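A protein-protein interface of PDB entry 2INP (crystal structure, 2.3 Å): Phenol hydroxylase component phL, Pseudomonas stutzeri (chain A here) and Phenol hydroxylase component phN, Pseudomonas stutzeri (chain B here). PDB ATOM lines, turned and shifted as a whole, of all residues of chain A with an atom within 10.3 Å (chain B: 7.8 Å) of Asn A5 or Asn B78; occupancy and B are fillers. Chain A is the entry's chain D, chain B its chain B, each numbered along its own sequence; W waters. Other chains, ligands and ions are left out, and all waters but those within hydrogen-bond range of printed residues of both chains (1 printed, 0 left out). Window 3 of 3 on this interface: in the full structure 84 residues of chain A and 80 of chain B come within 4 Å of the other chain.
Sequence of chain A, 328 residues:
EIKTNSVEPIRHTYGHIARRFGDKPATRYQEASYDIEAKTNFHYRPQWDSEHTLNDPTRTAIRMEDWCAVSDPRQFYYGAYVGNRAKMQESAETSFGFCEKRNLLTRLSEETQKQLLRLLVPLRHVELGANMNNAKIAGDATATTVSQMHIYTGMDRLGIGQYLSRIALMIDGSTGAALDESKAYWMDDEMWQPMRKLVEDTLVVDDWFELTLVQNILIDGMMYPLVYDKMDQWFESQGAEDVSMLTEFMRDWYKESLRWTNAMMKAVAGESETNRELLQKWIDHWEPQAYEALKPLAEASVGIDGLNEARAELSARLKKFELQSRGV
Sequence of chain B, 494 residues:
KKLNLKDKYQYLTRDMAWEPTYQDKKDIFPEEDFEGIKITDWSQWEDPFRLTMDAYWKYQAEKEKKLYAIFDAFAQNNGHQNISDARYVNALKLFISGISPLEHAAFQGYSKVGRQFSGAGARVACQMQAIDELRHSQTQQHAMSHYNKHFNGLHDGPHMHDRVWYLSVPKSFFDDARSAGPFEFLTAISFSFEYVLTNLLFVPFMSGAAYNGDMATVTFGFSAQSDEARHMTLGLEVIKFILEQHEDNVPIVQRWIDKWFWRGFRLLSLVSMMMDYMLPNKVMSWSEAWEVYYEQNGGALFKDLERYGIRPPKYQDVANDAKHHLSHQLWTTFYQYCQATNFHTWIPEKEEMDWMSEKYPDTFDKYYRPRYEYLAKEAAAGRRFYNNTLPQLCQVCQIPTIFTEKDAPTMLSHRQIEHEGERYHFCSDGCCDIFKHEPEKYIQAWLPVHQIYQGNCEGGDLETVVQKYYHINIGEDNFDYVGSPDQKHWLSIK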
ATOM      1  N   ILE A   2     -25.688  29.918  -5.863  1.00  0.00           N
ATOM      2  CA  ILE A   2     -24.987  28.954  -6.738  1.00  0.00           C
ATOM      3  C   ILE A   2     -24.671  29.608  -8.108  1.00  0.00           C
ATOM      4  O   ILE A   2     -25.579  30.119  -8.797  1.00  0.00           O
ATOM      5  CB  ILE A   2     -25.789  27.624  -6.934  1.00  0.00           C
ATOM      6  CG1 ILE A   2     -25.879  26.851  -5.607  1.00  0.00           C
ATOM      7  CG2 ILE A   2     -25.178  26.786  -8.075  1.00  0.00           C
ATOM      8  CD1 ILE A   2     -27.138  26.032  -5.469  1.00  0.00           C
ATOM      9  N   LYS A   3     -23.378  29.626  -8.452  1.00  0.00           N
ATOM     10  CA  LYS A   3     -22.911  30.046  -9.790  1.00  0.00           C
ATOM     11  C   LYS A   3     -23.194  28.945 -10.847  1.00  0.00           C
ATOM     12  O   LYS A   3     -22.941  27.760 -10.606  1.00  0.00           O
ATOM     13  CB  LYS A   3     -21.425  30.430  -9.759  1.00  0.00           C
ATOM     14  CG  LYS A   3     -21.098  31.508  -8.762  1.00  0.00           C
ATOM     15  CD  LYS A   3     -19.726  32.036  -9.041  1.00  0.00           C
ATOM     16  CE  LYS A   3     -19.493  33.342  -8.323  1.00  0.00           C
ATOM     17  NZ  LYS A   3     -18.169  33.913  -8.726  1.00  0.00           N
ATOM     18  N   THR A   4     -23.763  29.343 -11.989  1.00  0.00           N
ATOM     19  CA  THR A   4     -24.004  28.428 -13.111  1.00  0.00           C
ATOM     20  C   THR A   4     -23.234  28.929 -14.327  1.00  0.00           C
ATOM     21  O   THR A   4     -22.871  30.125 -14.398  1.00  0.00           O
ATOM     22  CB  THR A   4     -25.513  28.266 -13.474  1.00  0.00           C
ATOM     23  OG1 THR A   4     -26.344  28.697 -12.393  1.00  0.00           O
ATOM     24  CG2 THR A   4     -25.842  26.787 -13.810  1.00  0.00           C
ATOM     25  N   ASN A   5     -22.950  27.999 -15.246  1.00  0.00           N
ATOM     26  CA  ASN A   5     -22.412  28.348 -16.563  1.00  0.00           C
ATOM     27  C   ASN A   5     -23.529  28.834 -17.484  1.00  0.00           C
ATOM     28  O   ASN A   5     -24.465  28.058 -17.819  1.00  0.00           O
ATOM     29  CB  ASN A   5     -21.690  27.163 -17.187  1.00  0.00           C
ATOM     30  CG  ASN A   5     -20.195  27.382 -17.262  1.00  0.00           C
ATOM     31  OD1 ASN A   5     -19.731  28.500 -17.562  1.00  0.00           O
ATOM     32  ND2 ASN A   5     -19.419  26.310 -17.003  1.00  0.00           N
ATOM     33  N   SER A   6     -23.477  30.111 -17.864  1.00  0.00           N
ATOM     34  CA  SER A   6     -24.580  30.661 -18.665  1.00  0.00           C
ATOM     35  C   SER A   6     -24.149  30.881 -20.129  1.00  0.00           C
ATOM     36  O   SER A   6     -23.141  31.541 -20.410  1.00  0.00           O
ATOM     37  CB  SER A   6     -25.256  31.878 -17.998  1.00  0.00           C
ATOM     38  OG  SER A   6     -24.639  33.093 -18.379  1.00  0.00           O
ATOM     39  N   VAL A   7     -24.919  30.279 -21.032  1.00  0.00           N
ATOM     40  CA  VAL A   7     -24.550  30.108 -22.435  1.00  0.00           C
ATOM     41  C   VAL A   7     -25.268  31.110 -23.360  1.00  0.00           C
ATOM     42  O   VAL A   7     -26.423  31.488 -23.097  1.00  0.00           O
ATOM     43  CB  VAL A   7     -24.777  28.633 -22.865  1.00  0.00           C
ATOM     44  CG1 VAL A   7     -24.684  28.454 -24.419  1.00  0.00           C
ATOM     45  CG2 VAL A   7     -23.785  27.696 -22.058  1.00  0.00           C
ATOM     46  N   GLU A   8     -24.580  31.555 -24.418  1.00  0.00           N
ATOM     47  CA  GLU A   8     -25.138  32.590 -25.294  1.00  0.00           C
ATOM     48  C   GLU A   8     -26.093  32.034 -26.347  1.00  0.00           C
ATOM     49  O   GLU A   8     -25.685  31.257 -27.189  1.00  0.00           O
ATOM     50  CB  GLU A   8     -24.032  33.439 -25.933  1.00  0.00           C
ATOM     51  CG  GLU A   8     -23.674  34.667 -25.107  1.00  0.00           C
ATOM     52  CD  GLU A   8     -24.887  35.586 -24.858  1.00  0.00           C
ATOM     53  OE1 GLU A   8     -25.165  35.912 -23.672  1.00  0.00           O
ATOM     54  OE2 GLU A   8     -25.566  35.977 -25.848  1.00  0.00           O
ATOM     55  N   PRO A   9     -27.371  32.445 -26.286  1.00  0.00           N
ATOM     56  CA  PRO A   9     -28.340  31.923 -27.255  1.00  0.00           C
ATOM     57  C   PRO A   9     -28.292  32.725 -28.579  1.00  0.00           C
ATOM     58  O   PRO A   9     -27.888  33.904 -28.579  1.00  0.00           O
ATOM     59  CB  PRO A   9     -29.684  32.104 -26.537  1.00  0.00           C
ATOM     60  CG  PRO A   9     -29.464  33.269 -25.560  1.00  0.00           C
ATOM     61  CD  PRO A   9     -27.975  33.431 -25.352  1.00  0.00           C
ATOM     62  N   ILE A  10     -28.707  32.080 -29.677  1.00  0.00           N
ATOM     63  CA  ILE A  10     -28.915  32.748 -30.974  1.00  0.00           C
ATOM     64  C   ILE A  10     -30.118  33.641 -30.911  1.00  0.00           C
ATOM     65  O   ILE A  10     -30.153  34.724 -31.542  1.00  0.00           O
ATOM     66  CB  ILE A  10     -29.193  31.739 -32.114  1.00  0.00           C
ATOM     67  CG1 ILE A  10     -28.043  30.788 -32.287  1.00  0.00           C
ATOM     68  CG2 ILE A  10     -29.445  32.460 -33.449  1.00  0.00           C
ATOM     69  CD1 ILE A  10     -28.476  29.612 -33.065  1.00  0.00           C
ATOM     70  N   PHE B  71     -38.104  19.825 -17.834  1.00  0.00           N
ATOM     71  CA  PHE B  71     -37.865  20.850 -18.847  1.00  0.00           C
ATOM     72  C   PHE B  71     -37.069  22.029 -18.244  1.00  0.00           C
ATOM     73  O   PHE B  71     -36.081  22.484 -18.833  1.00  0.00           O
ATOM     74  CB  PHE B  71     -39.206  21.419 -19.286  1.00  0.00           C
ATOM     75  CG  PHE B  71     -39.990  20.540 -20.231  1.00  0.00           C
ATOM     76  CD1 PHE B  71     -39.409  19.351 -20.793  1.00  0.00           C
ATOM     77  CD2 PHE B  71     -41.311  20.912 -20.590  1.00  0.00           C
ATOM     78  CE1 PHE B  71     -40.088  18.605 -21.716  1.00  0.00           C
ATOM     79  CE2 PHE B  71     -42.045  20.121 -21.531  1.00  0.00           C
ATOM     80  CZ  PHE B  71     -41.416  18.976 -22.107  1.00  0.00           C
ATOM     81  N   ASP B  72     -37.526  22.548 -17.084  1.00  0.00           N
ATOM     82  CA  ASP B  72     -36.801  23.618 -16.365  1.00  0.00           C
ATOM     83  C   ASP B  72     -35.363  23.221 -16.060  1.00  0.00           C
ATOM     84  O   ASP B  72     -34.458  24.051 -16.233  1.00  0.00           O
ATOM     85  CB  ASP B  72     -37.499  24.040 -15.041  1.00  0.00           C
ATOM     86  CG  ASP B  72     -38.861  24.757 -15.273  1.00  0.00           C
ATOM     87  OD1 ASP B  72     -39.654  24.884 -14.300  1.00  0.00           O
ATOM     88  OD2 ASP B  72     -39.159  25.190 -16.416  1.00  0.00           O
ATOM     89  N   ALA B  73     -35.161  21.988 -15.587  1.00  0.00           N
ATOM     90  CA  ALA B  73     -33.810  21.517 -15.251  1.00  0.00           C
ATOM     91  C   ALA B  73     -32.930  21.327 -16.488  1.00  0.00           C
ATOM     92  O   ALA B  73     -31.763  21.741 -16.470  1.00  0.00           O
ATOM     93  CB  ALA B  73     -33.852  20.206 -14.424  1.00  0.00           C
ATOM     94  N   PHE B  74     -33.469  20.697 -17.546  1.00  0.00           N
ATOM     95  CA  PHE B  74     -32.793  20.650 -18.816  1.00  0.00           C
ATOM     96  C   PHE B  74     -32.296  22.025 -19.332  1.00  0.00           C
ATOM     97  O   PHE B  74     -31.175  22.183 -19.796  1.00  0.00           O
ATOM     98  CB  PHE B  74     -33.760  20.035 -19.827  1.00  0.00           C
ATOM     99  CG  PHE B  74     -33.160  19.774 -21.177  1.00  0.00           C
ATOM    100  CD1 PHE B  74     -32.455  18.577 -21.420  1.00  0.00           C
ATOM    101  CD2 PHE B  74     -33.267  20.729 -22.202  1.00  0.00           C
ATOM    102  CE1 PHE B  74     -31.891  18.328 -22.716  1.00  0.00           C
ATOM    103  CE2 PHE B  74     -32.718  20.476 -23.490  1.00  0.00           C
ATOM    104  CZ  PHE B  74     -32.024  19.298 -23.708  1.00  0.00           C
ATOM    105  N   ALA B  75     -33.145  23.037 -19.256  1.00  0.00           N
ATOM    106  CA  ALA B  75     -32.758  24.385 -19.707  1.00  0.00           C
ATOM    107  C   ALA B  75     -31.645  25.003 -18.850  1.00  0.00           C
ATOM    108  O   ALA B  75     -30.627  25.461 -19.388  1.00  0.00           O
ATOM    109  CB  ALA B  75     -33.956  25.296 -19.767  1.00  0.00           C
ATOM    110  N   GLN B  76     -31.817  24.934 -17.512  1.00  0.00           N
ATOM    111  CA  GLN B  76     -30.924  25.572 -16.532  1.00  0.00           C
ATOM    112  C   GLN B  76     -29.570  24.951 -16.674  1.00  0.00           C
ATOM    113  O   GLN B  76     -28.509  25.583 -16.513  1.00  0.00           O
ATOM    114  CB  GLN B  76     -31.477  25.320 -15.116  1.00  0.00           C
ATOM    115  CG  GLN B  76     -31.560  26.612 -14.233  1.00  0.00           C
ATOM    116  CD  GLN B  76     -30.190  26.975 -13.704  1.00  0.00           C
ATOM    117  OE1 GLN B  76     -29.734  28.139 -13.791  1.00  0.00           O
ATOM    118  NE2 GLN B  76     -29.479  25.951 -13.196  1.00  0.00           N
ATOM    119  N   ASN B  77     -29.602  23.685 -17.000  1.00  0.00           N
ATOM    120  CA  ASN B  77     -28.377  22.951 -17.087  1.00  0.00           C
ATOM    121  C   ASN B  77     -27.824  22.879 -18.528  1.00  0.00           C
ATOM    122  O   ASN B  77     -26.828  22.206 -18.763  1.00  0.00           O
ATOM    123  CB  ASN B  77     -28.570  21.580 -16.430  1.00  0.00           C
ATOM    124  CG  ASN B  77     -28.731  21.724 -14.874  1.00  0.00           C
ATOM    125  OD1 ASN B  77     -27.736  22.093 -14.208  1.00  0.00           O
ATOM    126  ND2 ASN B  77     -30.002  21.591 -14.326  1.00  0.00           N
ATOM    127  N   ASN B  78     -28.440  23.596 -19.475  1.00  0.00           N
ATOM    128  CA  ASN B  78     -27.921  23.526 -20.894  1.00  0.00           C
ATOM    129  C   ASN B  78     -27.842  22.104 -21.440  1.00  0.00           C
ATOM    130  O   ASN B  78     -26.833  21.696 -21.981  1.00  0.00           O
ATOM    131  CB  ASN B  78     -26.619  24.327 -21.061  1.00  0.00           C
ATOM    132  CG  ASN B  78     -26.888  25.850 -20.936  1.00  0.00           C
ATOM    133  OD1 ASN B  78     -27.832  26.400 -21.572  1.00  0.00           O
ATOM    134  ND2 ASN B  78     -26.128  26.521 -20.076  1.00  0.00           N
ATOM    135  N   GLY B  79     -28.904  21.326 -21.230  1.00  0.00           N
ATOM    136  CA  GLY B  79     -28.836  19.937 -21.632  1.00  0.00           C
ATOM    137  C   GLY B  79     -28.764  19.747 -23.141  1.00  0.00           C
ATOM    138  O   GLY B  79     -28.534  18.624 -23.602  1.00  0.00           O
ATOM    139  N   HIS B  80     -28.983  20.817 -23.913  1.00  0.00           N
ATOM    140  CA  HIS B  80     -28.823  20.724 -25.386  1.00  0.00           C
ATOM    141  C   HIS B  80     -27.361  20.368 -25.748  1.00  0.00           C
ATOM    142  O   HIS B  80     -27.071  19.807 -26.798  1.00  0.00           O
ATOM    143  CB  HIS B  80     -29.244  22.006 -26.073  1.00  0.00           C
ATOM    144  CG  HIS B  80     -28.376  23.167 -25.730  1.00  0.00           C
ATOM    145  ND1 HIS B  80     -28.505  23.866 -24.540  1.00  0.00           N
ATOM    146  CD2 HIS B  80     -27.395  23.794 -26.433  1.00  0.00           C
ATOM    147  CE1 HIS B  80     -27.631  24.857 -24.524  1.00  0.00           C
ATOM    148  NE2 HIS B  80     -26.927  24.811 -25.641  1.00  0.00           N
ATOM    149  N   GLN B  81     -26.445  20.655 -24.843  1.00  0.00           N
ATOM    150  CA  GLN B  81     -25.047  20.366 -25.035  1.00  0.00           C
ATOM    151  C   GLN B  81     -24.725  18.922 -24.809  1.00  0.00           C
ATOM    152  O   GLN B  81     -23.626  18.532 -25.096  1.00  0.00           O
ATOM    153  CB  GLN B  81     -24.241  21.246 -24.116  1.00  0.00           C
ATOM    154  CG  GLN B  81     -24.260  22.618 -24.704  1.00  0.00           C
ATOM    155  CD  GLN B  81     -23.471  23.611 -23.932  1.00  0.00           C
ATOM    156  OE1 GLN B  81     -23.441  23.586 -22.692  1.00  0.00           O
ATOM    157  NE2 GLN B  81     -22.847  24.547 -24.656  1.00  0.00           N
ATOM    158  N   ASN B  82     -25.699  18.121 -24.348  1.00  0.00           N
ATOM    159  CA  ASN B  82     -25.467  16.699 -24.045  1.00  0.00           C
ATOM    160  C   ASN B  82     -25.887  15.708 -25.128  1.00  0.00           C
ATOM    161  O   ASN B  82     -25.748  14.498 -24.969  1.00  0.00           O
ATOM    162  CB  ASN B  82     -26.160  16.352 -22.708  1.00  0.00           C
ATOM    163  CG  ASN B  82     -25.565  17.125 -21.544  1.00  0.00           C
ATOM    164  OD1 ASN B  82     -26.302  17.495 -20.624  1.00  0.00           O
ATOM    165  ND2 ASN B  82     -24.225  17.403 -21.595  1.00  0.00           N
ATOM    166  N   ILE B  83     -26.375  16.222 -26.265  1.00  0.00           N
ATOM    167  CA  ILE B  83     -26.823  15.325 -27.383  1.00  0.00           C
ATOM    168  C   ILE B  83     -25.558  14.697 -28.046  1.00  0.00           C
ATOM    169  O   ILE B  83     -24.466  15.175 -27.827  1.00  0.00           O
ATOM    170  CB  ILE B  83     -27.762  16.090 -28.342  1.00  0.00           C
ATOM    171  CG1 ILE B  83     -27.054  17.341 -28.822  1.00  0.00           C
ATOM    172  CG2 ILE B  83     -28.928  16.585 -27.550  1.00  0.00           C
ATOM    173  CD1 ILE B  83     -27.724  18.237 -29.797  1.00  0.00           C
ATOM    174  N   HIS B 146     -35.931  25.431 -25.741  1.00  0.00           N
ATOM    175  CA  HIS B 146     -34.542  25.654 -25.431  1.00  0.00           C
ATOM    176  C   HIS B 146     -33.653  25.358 -26.651  1.00  0.00           C
ATOM    177  O   HIS B 146     -32.649  26.021 -26.858  1.00  0.00           O
ATOM    178  CB  HIS B 146     -34.101  24.783 -24.239  1.00  0.00           C
ATOM    179  CG  HIS B 146     -32.743  25.124 -23.710  1.00  0.00           C
ATOM    180  ND1 HIS B 146     -32.465  26.329 -23.079  1.00  0.00           N
ATOM    181  CD2 HIS B 146     -31.582  24.421 -23.723  1.00  0.00           C
ATOM    182  CE1 HIS B 146     -31.183  26.355 -22.763  1.00  0.00           C
ATOM    183  NE2 HIS B 146     -30.630  25.204 -23.116  1.00  0.00           N
ATOM    184  N   HIS B 150     -30.688  27.801 -29.141  1.00  0.00           N
ATOM    185  CA  HIS B 150     -29.269  27.476 -29.455  1.00  0.00           C
ATOM    186  C   HIS B 150     -28.974  26.947 -30.890  1.00  0.00           C
ATOM    187  O   HIS B 150     -27.797  26.729 -31.252  1.00  0.00           O
ATOM    188  CB  HIS B 150     -28.679  26.527 -28.342  1.00  0.00           C
ATOM    189  CG  HIS B 150     -28.628  27.213 -27.021  1.00  0.00           C
ATOM    190  ND1 HIS B 150     -29.736  27.290 -26.188  1.00  0.00           N
ATOM    191  CD2 HIS B 150     -27.690  28.031 -26.486  1.00  0.00           C
ATOM    192  CE1 HIS B 150     -29.470  28.105 -25.186  1.00  0.00           C
ATOM    193  NE2 HIS B 150     -28.235  28.556 -25.339  1.00  0.00           N
ATOM    194  N   TRP B 490     -21.615  23.897 -32.681  1.00  0.00           N
ATOM    195  CA  TRP B 490     -21.270  22.643 -32.045  1.00  0.00           C
ATOM    196  C   TRP B 490     -19.753  22.422 -31.821  1.00  0.00           C
ATOM    197  O   TRP B 490     -19.313  22.057 -30.708  1.00  0.00           O
ATOM    198  CB  TRP B 490     -21.837  21.469 -32.810  1.00  0.00           C
ATOM    199  CG  TRP B 490     -21.867  20.216 -32.048  1.00  0.00           C
ATOM    200  CD1 TRP B 490     -21.188  19.069 -32.339  1.00  0.00           C
ATOM    201  CD2 TRP B 490     -22.653  19.928 -30.874  1.00  0.00           C
ATOM    202  NE1 TRP B 490     -21.509  18.073 -31.415  1.00  0.00           N
ATOM    203  CE2 TRP B 490     -22.383  18.594 -30.499  1.00  0.00           C
ATOM    204  CE3 TRP B 490     -23.539  20.680 -30.087  1.00  0.00           C
ATOM    205  CZ2 TRP B 490     -22.972  18.005 -29.401  1.00  0.00           C
ATOM    206  CZ3 TRP B 490     -24.112  20.086 -29.003  1.00  0.00           C
ATOM    207  CH2 TRP B 490     -23.828  18.763 -28.672  1.00  0.00           C
HETATM  208  O   HOH W   1     -28.510  29.125 -22.515  1.00  0.00           O
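Of chain B, only Asn B78 (3.2 Å) comes within 4 Å of Asn A5.
Of the printed residues of chain B, Val A7 touches Asn B78 (3.3 Å) and His B150 (3.7 Å).
Of the printed residues of chain B, Glu A8 touches His B150 (3.9 Å).
No residue of chain A comes within 4 Å of Ala B75.
No residue of chain A comes within 4 Å of Asn B77.
Of the printed residues of chain A, Asn B78 touches Asn A5 (3.2 Å) and Val A7 (3.3 Å).
No residue of chain A comes within 4 Å of Gly B79.
No residue of chain A comes within 4 Å of Gln B81.
The nearest residue of chain B that does not touch Asn A5 is Gln B76 (4.9 Å).
The nearest residue of chain A that does not touch Asn B78 is Ser A6 (4.6 Å).
The nearest printed residue of chain B that does not touch Ile A10 is His B146 (7.8 Å).
Among the printed residues, merely in contact across the chains: Val A7 with Asn B78, Ile A10 with His B150, Val A7 with His B150, Thr A4 with Gln B76, Glu A8 with His B150 and Pro A9 with His B150.
NE2 of His B146 lies within hydrogen-bond range of OD1 of Asn B78 (3.4 Å).
ND1 of His B150 lies within hydrogen-bond range of O of His B146 (3.2 Å).
Water W1 lies within hydrogen-bond range of NE2 of His B150 (2.9 Å), OD1 of Asn B78 (3.0 Å) and O of Val A7 (3.2 Å).
O of Asn A5 is in hydrogen-bond range of ND2 of Asn B78, 3.2 Å away.
Of the 16 printed residues of chain B, 3 touch a printed residue of chain A.
Among the printed residues, 7 pairs touch across the chains.
Among the printed residues, no Asp or Glu carboxylate lies within 4 Å of a Lys or Arg side-chain nitrogen of the other chain.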
